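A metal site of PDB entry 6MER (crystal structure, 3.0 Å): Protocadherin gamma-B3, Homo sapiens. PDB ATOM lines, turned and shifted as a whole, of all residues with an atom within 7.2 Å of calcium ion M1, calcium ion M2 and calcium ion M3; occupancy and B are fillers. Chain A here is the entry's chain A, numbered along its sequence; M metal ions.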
ATOM      1  N   GLU A 114      16.811  14.626  -6.242  1.00  0.00           N
ATOM      2  CA  GLU A 114      18.138  15.229  -6.171  1.00  0.00           C
ATOM      3  C   GLU A 114      18.087  16.752  -6.190  1.00  0.00           C
ATOM      4  O   GLU A 114      19.039  17.390  -5.715  1.00  0.00           O
ATOM      5  CB  GLU A 114      19.000  14.734  -7.333  1.00  0.00           C
ATOM      6  CG  GLU A 114      19.068  13.228  -7.482  1.00  0.00           C
ATOM      7  CD  GLU A 114      19.957  12.798  -8.630  1.00  0.00           C
ATOM      8  OE1 GLU A 114      21.009  13.438  -8.839  1.00  0.00           O
ATOM      9  OE2 GLU A 114      19.615  11.824  -9.327  1.00  0.00           O
ATOM     10  N   LEU A 170      21.812  16.223  -2.406  1.00  0.00           N
ATOM     11  CA  LEU A 170      21.633  14.790  -2.649  1.00  0.00           C
ATOM     12  C   LEU A 170      22.006  14.454  -4.079  1.00  0.00           C
ATOM     13  O   LEU A 170      21.519  15.091  -5.024  1.00  0.00           O
ATOM     14  CB  LEU A 170      20.194  14.373  -2.369  1.00  0.00           C
ATOM     15  CG  LEU A 170      19.741  14.382  -0.900  1.00  0.00           C
ATOM     16  CD1 LEU A 170      18.328  13.856  -0.769  1.00  0.00           C
ATOM     17  CD2 LEU A 170      20.711  13.578  -0.041  1.00  0.00           C
ATOM     18  N   ASP A 171      22.867  13.458  -4.247  1.00  0.00           N
ATOM     19  CA  ASP A 171      23.289  12.966  -5.553  1.00  0.00           C
ATOM     20  C   ASP A 171      22.993  11.471  -5.606  1.00  0.00           C
ATOM     21  O   ASP A 171      23.697  10.685  -4.960  1.00  0.00           O
ATOM     22  CB  ASP A 171      24.764  13.258  -5.802  1.00  0.00           C
ATOM     23  CG  ASP A 171      25.197  12.944  -7.227  1.00  0.00           C
ATOM     24  OD1 ASP A 171      24.338  12.538  -8.033  1.00  0.00           O
ATOM     25  OD2 ASP A 171      26.392  13.115  -7.532  1.00  0.00           O
ATOM     26  N   ARG A 172      21.966  11.086  -6.347  1.00  0.00           N
ATOM     27  CA  ARG A 172      21.615   9.675  -6.458  1.00  0.00           C
ATOM     28  C   ARG A 172      22.723   8.881  -7.135  1.00  0.00           C
ATOM     29  O   ARG A 172      22.937   7.706  -6.800  1.00  0.00           O
ATOM     30  CB  ARG A 172      20.308   9.508  -7.227  1.00  0.00           C
ATOM     31  CG  ARG A 172      19.760   8.084  -7.232  1.00  0.00           C
ATOM     32  CD  ARG A 172      18.843   7.851  -8.417  1.00  0.00           C
ATOM     33  NE  ARG A 172      19.570   7.914  -9.688  1.00  0.00           N
ATOM     34  CZ  ARG A 172      20.139   6.868 -10.272  1.00  0.00           C
ATOM     35  NH1 ARG A 172      20.072   5.673  -9.707  1.00  0.00           N
ATOM     36  NH2 ARG A 172      20.782   7.014 -11.424  1.00  0.00           N
ATOM     37  N   GLU A 173      23.436   9.500  -8.074  1.00  0.00           N
ATOM     38  CA  GLU A 173      24.550   8.823  -8.743  1.00  0.00           C
ATOM     39  C   GLU A 173      25.724   8.561  -7.813  1.00  0.00           C
ATOM     40  O   GLU A 173      26.610   7.786  -8.171  1.00  0.00           O
ATOM     41  CB  GLU A 173      25.011   9.647  -9.946  1.00  0.00           C
ATOM     42  CG  GLU A 173      24.044   9.646 -11.125  1.00  0.00           C
ATOM     43  CD  GLU A 173      22.763  10.411 -10.854  1.00  0.00           C
ATOM     44  OE1 GLU A 173      22.823  11.468 -10.189  1.00  0.00           O
ATOM     45  OE2 GLU A 173      21.683   9.955 -11.295  1.00  0.00           O
ATOM     46  N   GLU A 174      25.747   9.193  -6.642  1.00  0.00           N
ATOM     47  CA  GLU A 174      26.763   8.936  -5.622  1.00  0.00           C
ATOM     48  C   GLU A 174      26.261   8.056  -4.496  1.00  0.00           C
ATOM     49  O   GLU A 174      27.004   7.192  -4.007  1.00  0.00           O
ATOM     50  CB  GLU A 174      27.277  10.264  -5.056  1.00  0.00           C
ATOM     51  CG  GLU A 174      28.341  10.128  -3.976  1.00  0.00           C
ATOM     52  CD  GLU A 174      29.669   9.627  -4.518  1.00  0.00           C
ATOM     53  OE1 GLU A 174      29.904   9.754  -5.748  1.00  0.00           O
ATOM     54  OE2 GLU A 174      30.476   9.107  -3.730  1.00  0.00           O
ATOM     55  N   ALA A 203      15.267  10.124  -4.975  1.00  0.00           N
ATOM     56  CA  ALA A 203      14.604  10.004  -6.260  1.00  0.00           C
ATOM     57  C   ALA A 203      15.476  10.597  -7.364  1.00  0.00           C
ATOM     58  O   ALA A 203      16.166  11.600  -7.159  1.00  0.00           O
ATOM     59  CB  ALA A 203      13.247  10.701  -6.232  1.00  0.00           C
ATOM     60  N   ASP A 204      15.445   9.970  -8.532  1.00  0.00           N
ATOM     61  CA  ASP A 204      16.295  10.388  -9.634  1.00  0.00           C
ATOM     62  C   ASP A 204      15.777  11.684 -10.256  1.00  0.00           C
ATOM     63  O   ASP A 204      14.571  11.914 -10.344  1.00  0.00           O
ATOM     64  CB  ASP A 204      16.376   9.299 -10.707  1.00  0.00           C
ATOM     65  CG  ASP A 204      17.273   9.681 -11.860  1.00  0.00           C
ATOM     66  OD1 ASP A 204      18.501   9.759 -11.661  1.00  0.00           O
ATOM     67  OD2 ASP A 204      16.747   9.917 -12.967  1.00  0.00           O
ATOM     68  N   ALA A 205      16.711  12.537 -10.682  1.00  0.00           N
ATOM     69  CA  ALA A 205      16.408  13.773 -11.378  1.00  0.00           C
ATOM     70  C   ALA A 205      17.298  13.876 -12.609  1.00  0.00           C
ATOM     71  O   ALA A 205      18.489  13.565 -12.544  1.00  0.00           O
ATOM     72  CB  ALA A 205      16.601  14.989 -10.477  1.00  0.00           C
ATOM     73  N   ASN A 206      16.714  14.315 -13.721  1.00  0.00           N
ATOM     74  CA  ASN A 206      17.439  14.414 -14.986  1.00  0.00           C
ATOM     75  C   ASN A 206      18.395  15.599 -14.918  1.00  0.00           C
ATOM     76  O   ASN A 206      18.122  16.705 -15.400  1.00  0.00           O
ATOM     77  CB  ASN A 206      16.474  14.548 -16.162  1.00  0.00           C
ATOM     78  CG  ASN A 206      17.179  14.561 -17.496  1.00  0.00           C
ATOM     79  OD1 ASN A 206      17.468  15.623 -18.058  1.00  0.00           O
ATOM     80  ND2 ASN A 206      17.452  13.376 -18.033  1.00  0.00           N
ATOM     81  N   ASP A 207      19.562  15.353 -14.309  1.00  0.00           N
ATOM     82  CA  ASP A 207      20.601  16.375 -14.187  1.00  0.00           C
ATOM     83  C   ASP A 207      21.893  15.984 -14.886  1.00  0.00           C
ATOM     84  O   ASP A 207      22.836  16.792 -14.894  1.00  0.00           O
ATOM     85  CB  ASP A 207      20.883  16.680 -12.706  1.00  0.00           C
ATOM     86  CG  ASP A 207      21.475  15.479 -11.971  1.00  0.00           C
ATOM     87  OD1 ASP A 207      21.200  14.334 -12.376  1.00  0.00           O
ATOM     88  OD2 ASP A 207      22.206  15.698 -10.986  1.00  0.00           O
ATOM     89  N   ASN A 208      21.973  14.791 -15.468  1.00  0.00           N
ATOM     90  CA  ASN A 208      23.162  14.347 -16.182  1.00  0.00           C
ATOM     91  C   ASN A 208      22.843  14.192 -17.661  1.00  0.00           C
ATOM     92  O   ASN A 208      22.182  13.222 -18.060  1.00  0.00           O
ATOM     93  CB  ASN A 208      23.682  13.021 -15.618  1.00  0.00           C
ATOM     94  CG  ASN A 208      24.246  13.172 -14.213  1.00  0.00           C
ATOM     95  OD1 ASN A 208      23.897  14.106 -13.485  1.00  0.00           O
ATOM     96  ND2 ASN A 208      25.118  12.252 -13.824  1.00  0.00           N
ATOM     97  N   PRO A 209      23.264  15.121 -18.520  1.00  0.00           N
ATOM     98  CA  PRO A 209      23.030  14.970 -19.958  1.00  0.00           C
ATOM     99  C   PRO A 209      23.810  13.804 -20.523  1.00  0.00           C
ATOM    100  O   PRO A 209      24.779  13.332 -19.900  1.00  0.00           O
ATOM    101  CB  PRO A 209      23.520  16.312 -20.544  1.00  0.00           C
ATOM    102  CG  PRO A 209      23.553  17.254 -19.380  1.00  0.00           C
ATOM    103  CD  PRO A 209      23.894  16.402 -18.190  1.00  0.00           C
ATOM    104  N   PRO A 210      23.428  13.296 -21.702  1.00  0.00           N
ATOM    105  CA  PRO A 210      24.204  12.216 -22.317  1.00  0.00           C
ATOM    106  C   PRO A 210      25.615  12.662 -22.658  1.00  0.00           C
ATOM    107  O   PRO A 210      25.865  13.840 -22.937  1.00  0.00           O
ATOM    108  CB  PRO A 210      23.396  11.879 -23.577  1.00  0.00           C
ATOM    109  CG  PRO A 210      22.008  12.368 -23.288  1.00  0.00           C
ATOM    110  CD  PRO A 210      22.187  13.592 -22.448  1.00  0.00           C
ATOM    111  N   ILE A 237      26.539   7.633 -22.734  1.00  0.00           N
ATOM    112  CA  ILE A 237      26.373   7.177 -21.358  1.00  0.00           C
ATOM    113  C   ILE A 237      25.521   8.193 -20.614  1.00  0.00           C
ATOM    114  O   ILE A 237      25.819   9.396 -20.622  1.00  0.00           O
ATOM    115  CB  ILE A 237      27.735   6.989 -20.672  1.00  0.00           C
ATOM    116  CG1 ILE A 237      28.530   5.870 -21.348  1.00  0.00           C
ATOM    117  CG2 ILE A 237      27.542   6.686 -19.194  1.00  0.00           C
ATOM    118  CD1 ILE A 237      27.857   4.526 -21.287  1.00  0.00           C
ATOM    119  N   ASP A 238      24.458   7.706 -19.976  1.00  0.00           N
ATOM    120  CA  ASP A 238      23.577   8.536 -19.157  1.00  0.00           C
ATOM    121  C   ASP A 238      23.512   7.908 -17.765  1.00  0.00           C
ATOM    122  O   ASP A 238      22.952   6.826 -17.597  1.00  0.00           O
ATOM    123  CB  ASP A 238      22.184   8.633 -19.783  1.00  0.00           C
ATOM    124  CG  ASP A 238      21.405   9.834 -19.279  1.00  0.00           C
ATOM    125  OD1 ASP A 238      21.505  10.152 -18.075  1.00  0.00           O
ATOM    126  OD2 ASP A 238      20.696  10.463 -20.092  1.00  0.00           O
ATOM    127  N   MET A 239      24.096   8.600 -16.781  1.00  0.00           N
ATOM    128  CA  MET A 239      24.221   8.064 -15.428  1.00  0.00           C
ATOM    129  C   MET A 239      22.924   8.109 -14.639  1.00  0.00           C
ATOM    130  O   MET A 239      22.914   7.675 -13.483  1.00  0.00           O
ATOM    131  CB  MET A 239      25.304   8.834 -14.675  1.00  0.00           C
ATOM    132  CG  MET A 239      26.690   8.758 -15.308  1.00  0.00           C
ATOM    133  SD  MET A 239      27.330   7.079 -15.355  1.00  0.00           S
ATOM    134  CE  MET A 239      27.376   6.679 -13.608  1.00  0.00           C
ATOM    135  N   ASP A 240      21.825   8.601 -15.222  1.00  0.00           N
ATOM    136  CA  ASP A 240      20.566   8.708 -14.496  1.00  0.00           C
ATOM    137  C   ASP A 240      19.851   7.358 -14.445  1.00  0.00           C
ATOM    138  O   ASP A 240      20.450   6.312 -14.693  1.00  0.00           O
ATOM    139  CB  ASP A 240      19.675   9.774 -15.127  1.00  0.00           C
ATOM    140  CG  ASP A 240      20.259  11.157 -15.011  1.00  0.00           C
ATOM    141  OD1 ASP A 240      21.067  11.400 -14.087  1.00  0.00           O
ATOM    142  OD2 ASP A 240      19.907  12.026 -15.843  1.00  0.00           O
ATOM    143  N   GLU A 241      18.556   7.381 -14.115  1.00  0.00           N
ATOM    144  CA  GLU A 241      17.786   6.167 -13.903  1.00  0.00           C
ATOM    145  C   GLU A 241      16.459   6.254 -14.646  1.00  0.00           C
ATOM    146  O   GLU A 241      15.777   7.282 -14.598  1.00  0.00           O
ATOM    147  CB  GLU A 241      17.525   5.929 -12.413  1.00  0.00           C
ATOM    148  CG  GLU A 241      16.609   4.760 -12.106  1.00  0.00           C
ATOM    149  CD  GLU A 241      16.257   4.654 -10.640  1.00  0.00           C
ATOM    150  OE1 GLU A 241      16.802   5.443  -9.841  1.00  0.00           O
ATOM    151  OE2 GLU A 241      15.415   3.796 -10.289  1.00  0.00           O
ATOM    152  N   ILE A 243      13.625   6.738 -17.265  1.00  0.00           N
ATOM    153  CA  ILE A 243      13.394   7.555 -18.456  1.00  0.00           C
ATOM    154  C   ILE A 243      14.500   8.586 -18.630  1.00  0.00           C
ATOM    155  O   ILE A 243      14.832   8.955 -19.771  1.00  0.00           O
ATOM    156  CB  ILE A 243      12.000   8.217 -18.375  1.00  0.00           C
ATOM    157  CG1 ILE A 243      11.734   9.093 -19.592  1.00  0.00           C
ATOM    158  CG2 ILE A 243      11.872   9.025 -17.083  1.00  0.00           C
ATOM    159  CD1 ILE A 243      11.755   8.339 -20.908  1.00  0.00           C
ATOM    160  N   ASN A 244      15.109   9.041 -17.533  1.00  0.00           N
ATOM    161  CA  ASN A 244      16.190  10.013 -17.610  1.00  0.00           C
ATOM    162  C   ASN A 244      17.498   9.407 -18.109  1.00  0.00           C
ATOM    163  O   ASN A 244      18.504  10.122 -18.174  1.00  0.00           O
ATOM    164  CB  ASN A 244      16.397  10.663 -16.247  1.00  0.00           C
ATOM    165  CG  ASN A 244      15.144  11.304 -15.704  1.00  0.00           C
ATOM    166  OD1 ASN A 244      14.282  11.749 -16.466  1.00  0.00           O
ATOM    167  ND2 ASN A 244      15.031  11.376 -14.385  1.00  0.00           N
ATOM    168  N   ALA A 245      17.514   8.114 -18.457  1.00  0.00           N
ATOM    169  CA  ALA A 245      18.702   7.469 -18.975  1.00  0.00           C
ATOM    170  C   ALA A 245      18.512   6.838 -20.353  1.00  0.00           C
ATOM    171  O   ALA A 245      19.506   6.463 -20.981  1.00  0.00           O
ATOM    172  CB  ALA A 245      19.201   6.399 -18.002  1.00  0.00           C
ATOM    173  N   GLU A 246      17.275   6.697 -20.821  1.00  0.00           N
ATOM    174  CA  GLU A 246      17.022   6.135 -22.142  1.00  0.00           C
ATOM    175  C   GLU A 246      17.420   7.160 -23.209  1.00  0.00           C
ATOM    176  O   GLU A 246      16.934   8.288 -23.196  1.00  0.00           O
ATOM    177  CB  GLU A 246      15.564   5.747 -22.286  1.00  0.00           C
ATOM    178  CG  GLU A 246      15.104   4.687 -21.284  1.00  0.00           C
ATOM    179  CD  GLU A 246      13.619   4.399 -21.383  1.00  0.00           C
ATOM    180  OE1 GLU A 246      12.921   5.093 -22.157  1.00  0.00           O
ATOM    181  OE2 GLU A 246      13.151   3.474 -20.682  1.00  0.00           O
ATOM    182  N   ILE A 247      18.296   6.746 -24.119  1.00  0.00           N
ATOM    183  CA  ILE A 247      18.878   7.636 -25.116  1.00  0.00           C
ATOM    184  C   ILE A 247      18.389   7.241 -26.501  1.00  0.00           C
ATOM    185  O   ILE A 247      18.326   6.054 -26.829  1.00  0.00           O
ATOM    186  CB  ILE A 247      20.416   7.603 -25.052  1.00  0.00           C
ATOM    187  CG1 ILE A 247      20.896   7.819 -23.613  1.00  0.00           C
ATOM    188  CG2 ILE A 247      21.021   8.652 -25.981  1.00  0.00           C
ATOM    189  CD1 ILE A 247      22.374   7.627 -23.429  1.00  0.00           C
ATOM    190  N   ASP A 293      17.491  12.391 -24.306  1.00  0.00           N
ATOM    191  CA  ASP A 293      16.879  11.531 -23.305  1.00  0.00           C
ATOM    192  C   ASP A 293      15.445  12.001 -23.021  1.00  0.00           C
ATOM    193  O   ASP A 293      14.885  12.837 -23.743  1.00  0.00           O
ATOM    194  CB  ASP A 293      17.723  11.486 -22.028  1.00  0.00           C
ATOM    195  CG  ASP A 293      17.959  12.872 -21.439  1.00  0.00           C
ATOM    196  OD1 ASP A 293      17.589  13.871 -22.091  1.00  0.00           O
ATOM    197  OD2 ASP A 293      18.502  12.946 -20.318  1.00  0.00           O
ATOM    198  N   GLY A 294      14.860  11.460 -21.948  1.00  0.00           N
ATOM    199  CA  GLY A 294      13.516  11.849 -21.574  1.00  0.00           C
ATOM    200  C   GLY A 294      13.422  13.283 -21.072  1.00  0.00           C
ATOM    201  O   GLY A 294      12.404  13.943 -21.259  1.00  0.00           O
ATOM    202  N   GLY A 295      14.487  13.767 -20.421  1.00  0.00           N
ATOM    203  CA  GLY A 295      14.538  15.120 -19.921  1.00  0.00           C
ATOM    204  C   GLY A 295      14.900  16.164 -20.944  1.00  0.00           C
ATOM    205  O   GLY A 295      15.190  17.311 -20.572  1.00  0.00           O
ATOM    206  N   HIS A 297      17.532  16.623 -22.547  1.00  0.00           N
ATOM    207  CA  HIS A 297      18.928  17.021 -22.547  1.00  0.00           C
ATOM    208  C   HIS A 297      19.617  16.472 -23.798  1.00  0.00           C
ATOM    209  O   HIS A 297      19.578  15.268 -24.059  1.00  0.00           O
ATOM    210  CB  HIS A 297      19.631  16.521 -21.284  1.00  0.00           C
ATOM    211  CG  HIS A 297      19.493  17.446 -20.115  1.00  0.00           C
ATOM    212  ND1 HIS A 297      20.167  17.245 -18.927  1.00  0.00           N
ATOM    213  CD2 HIS A 297      18.768  18.571 -19.955  1.00  0.00           C
ATOM    214  CE1 HIS A 297      19.857  18.208 -18.080  1.00  0.00           C
ATOM    215  NE2 HIS A 297      19.012  19.030 -18.678  1.00  0.00           N
HETATM  216 CA    CA M   1      23.281  13.883  -9.744  1.00  0.00          CA
HETATM  217 CA    CA M   2      20.163  11.904 -11.725  1.00  0.00          CA
HETATM  218 CA    CA M   3      19.915  12.201 -18.293  1.00  0.00          CA
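The backbone NH (N) of His 297 lies within hydrogen-bond range of the side-chain carboxylate (OD1) of Asp 293. O of Asp 240 lies close to NH2 of Arg 172. The backbone carbonyl oxygen (O) of Ala 203 is in hydrogen-bond range of the backbone NH (N) of Glu 114. The side-chain amide oxygen (OD1) of Asn 206 lies within hydrogen-bond range of a ring nitrogen (ND1) of His 297, at 3.3 Å. N of Glu 241 is in hydrogen-bond range of OD2 of Asp 204 (3.3 Å). The side-chain carboxylate (OE2) of Glu 173 lies close to the guanidinium group (NH2) of Arg 172 (3.1 Å). OE2 of Glu 114 lies close to NE of Arg 172. The guanidinium group of Arg 172 sits close to the side-chain carboxylate of Asp 204, at 2.9 Å.
Within 4 Å of calcium ion M1: Glu 114, Asp 171, Glu 173, Asp 207 and Asn 208.
Six residues have an atom within 4 Å of calcium ion M2: Glu 114, Glu 173, Asp 204, Ala 205, Asp 207 and Asp 240.
The nearest printed residue that does not touch calcium ion M3 is Pro 209 (4.4 Å).
Calcium ion M1 is bound by the side-chain carboxylate of Asp 171 (2.4 Å), the side-chain carboxylate of Asp 207 (2.4 Å), the side-chain carboxylate of Glu 114 (2.5 Å) and the side-chain carboxylate of Glu 173 (2.5 Å).
OE2 of Glu 114 binds calcium ion M2 (2.5 Å). O of Ala 205 binds calcium ion M2, 2.5 Å away. The side-chain carboxylate (OE2) of Glu 173 binds calcium ion M2. OD1 of Asp 240 is bound to calcium ion M2 (2.6 Å). Calcium ion M2 is bound by OD1 of Asp 204, 2.7 Å away. Calcium ion M2 is bound by OD1 of Asp 207 (2.7 Å). Slightly farther from calcium ion M2 lies the side-chain carboxylate (OE1) of Glu 173 (3.1 Å).
OD2 of Asp 240 is bound to calcium ion M3, at 2.5 Å. Calcium ion M3 is bound by O of Asn 208, 2.5 Å away. O of Asn 244 binds calcium ion M3 (2.5 Å). Calcium ion M3 is bound by the side-chain carboxylate (OD2) of Asp 293 (2.6 Å). Calcium ion M3 is bound by OD1 of Asp 238, 2.6 Å away. Calcium ion M3 is bound by the side-chain carboxylate (OD2) of Asp 238 (2.6 Å). Calcium ion M3 is bound by ND2 of Asn 206. Calcium ion M3 has seven donor atoms within binding distance.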
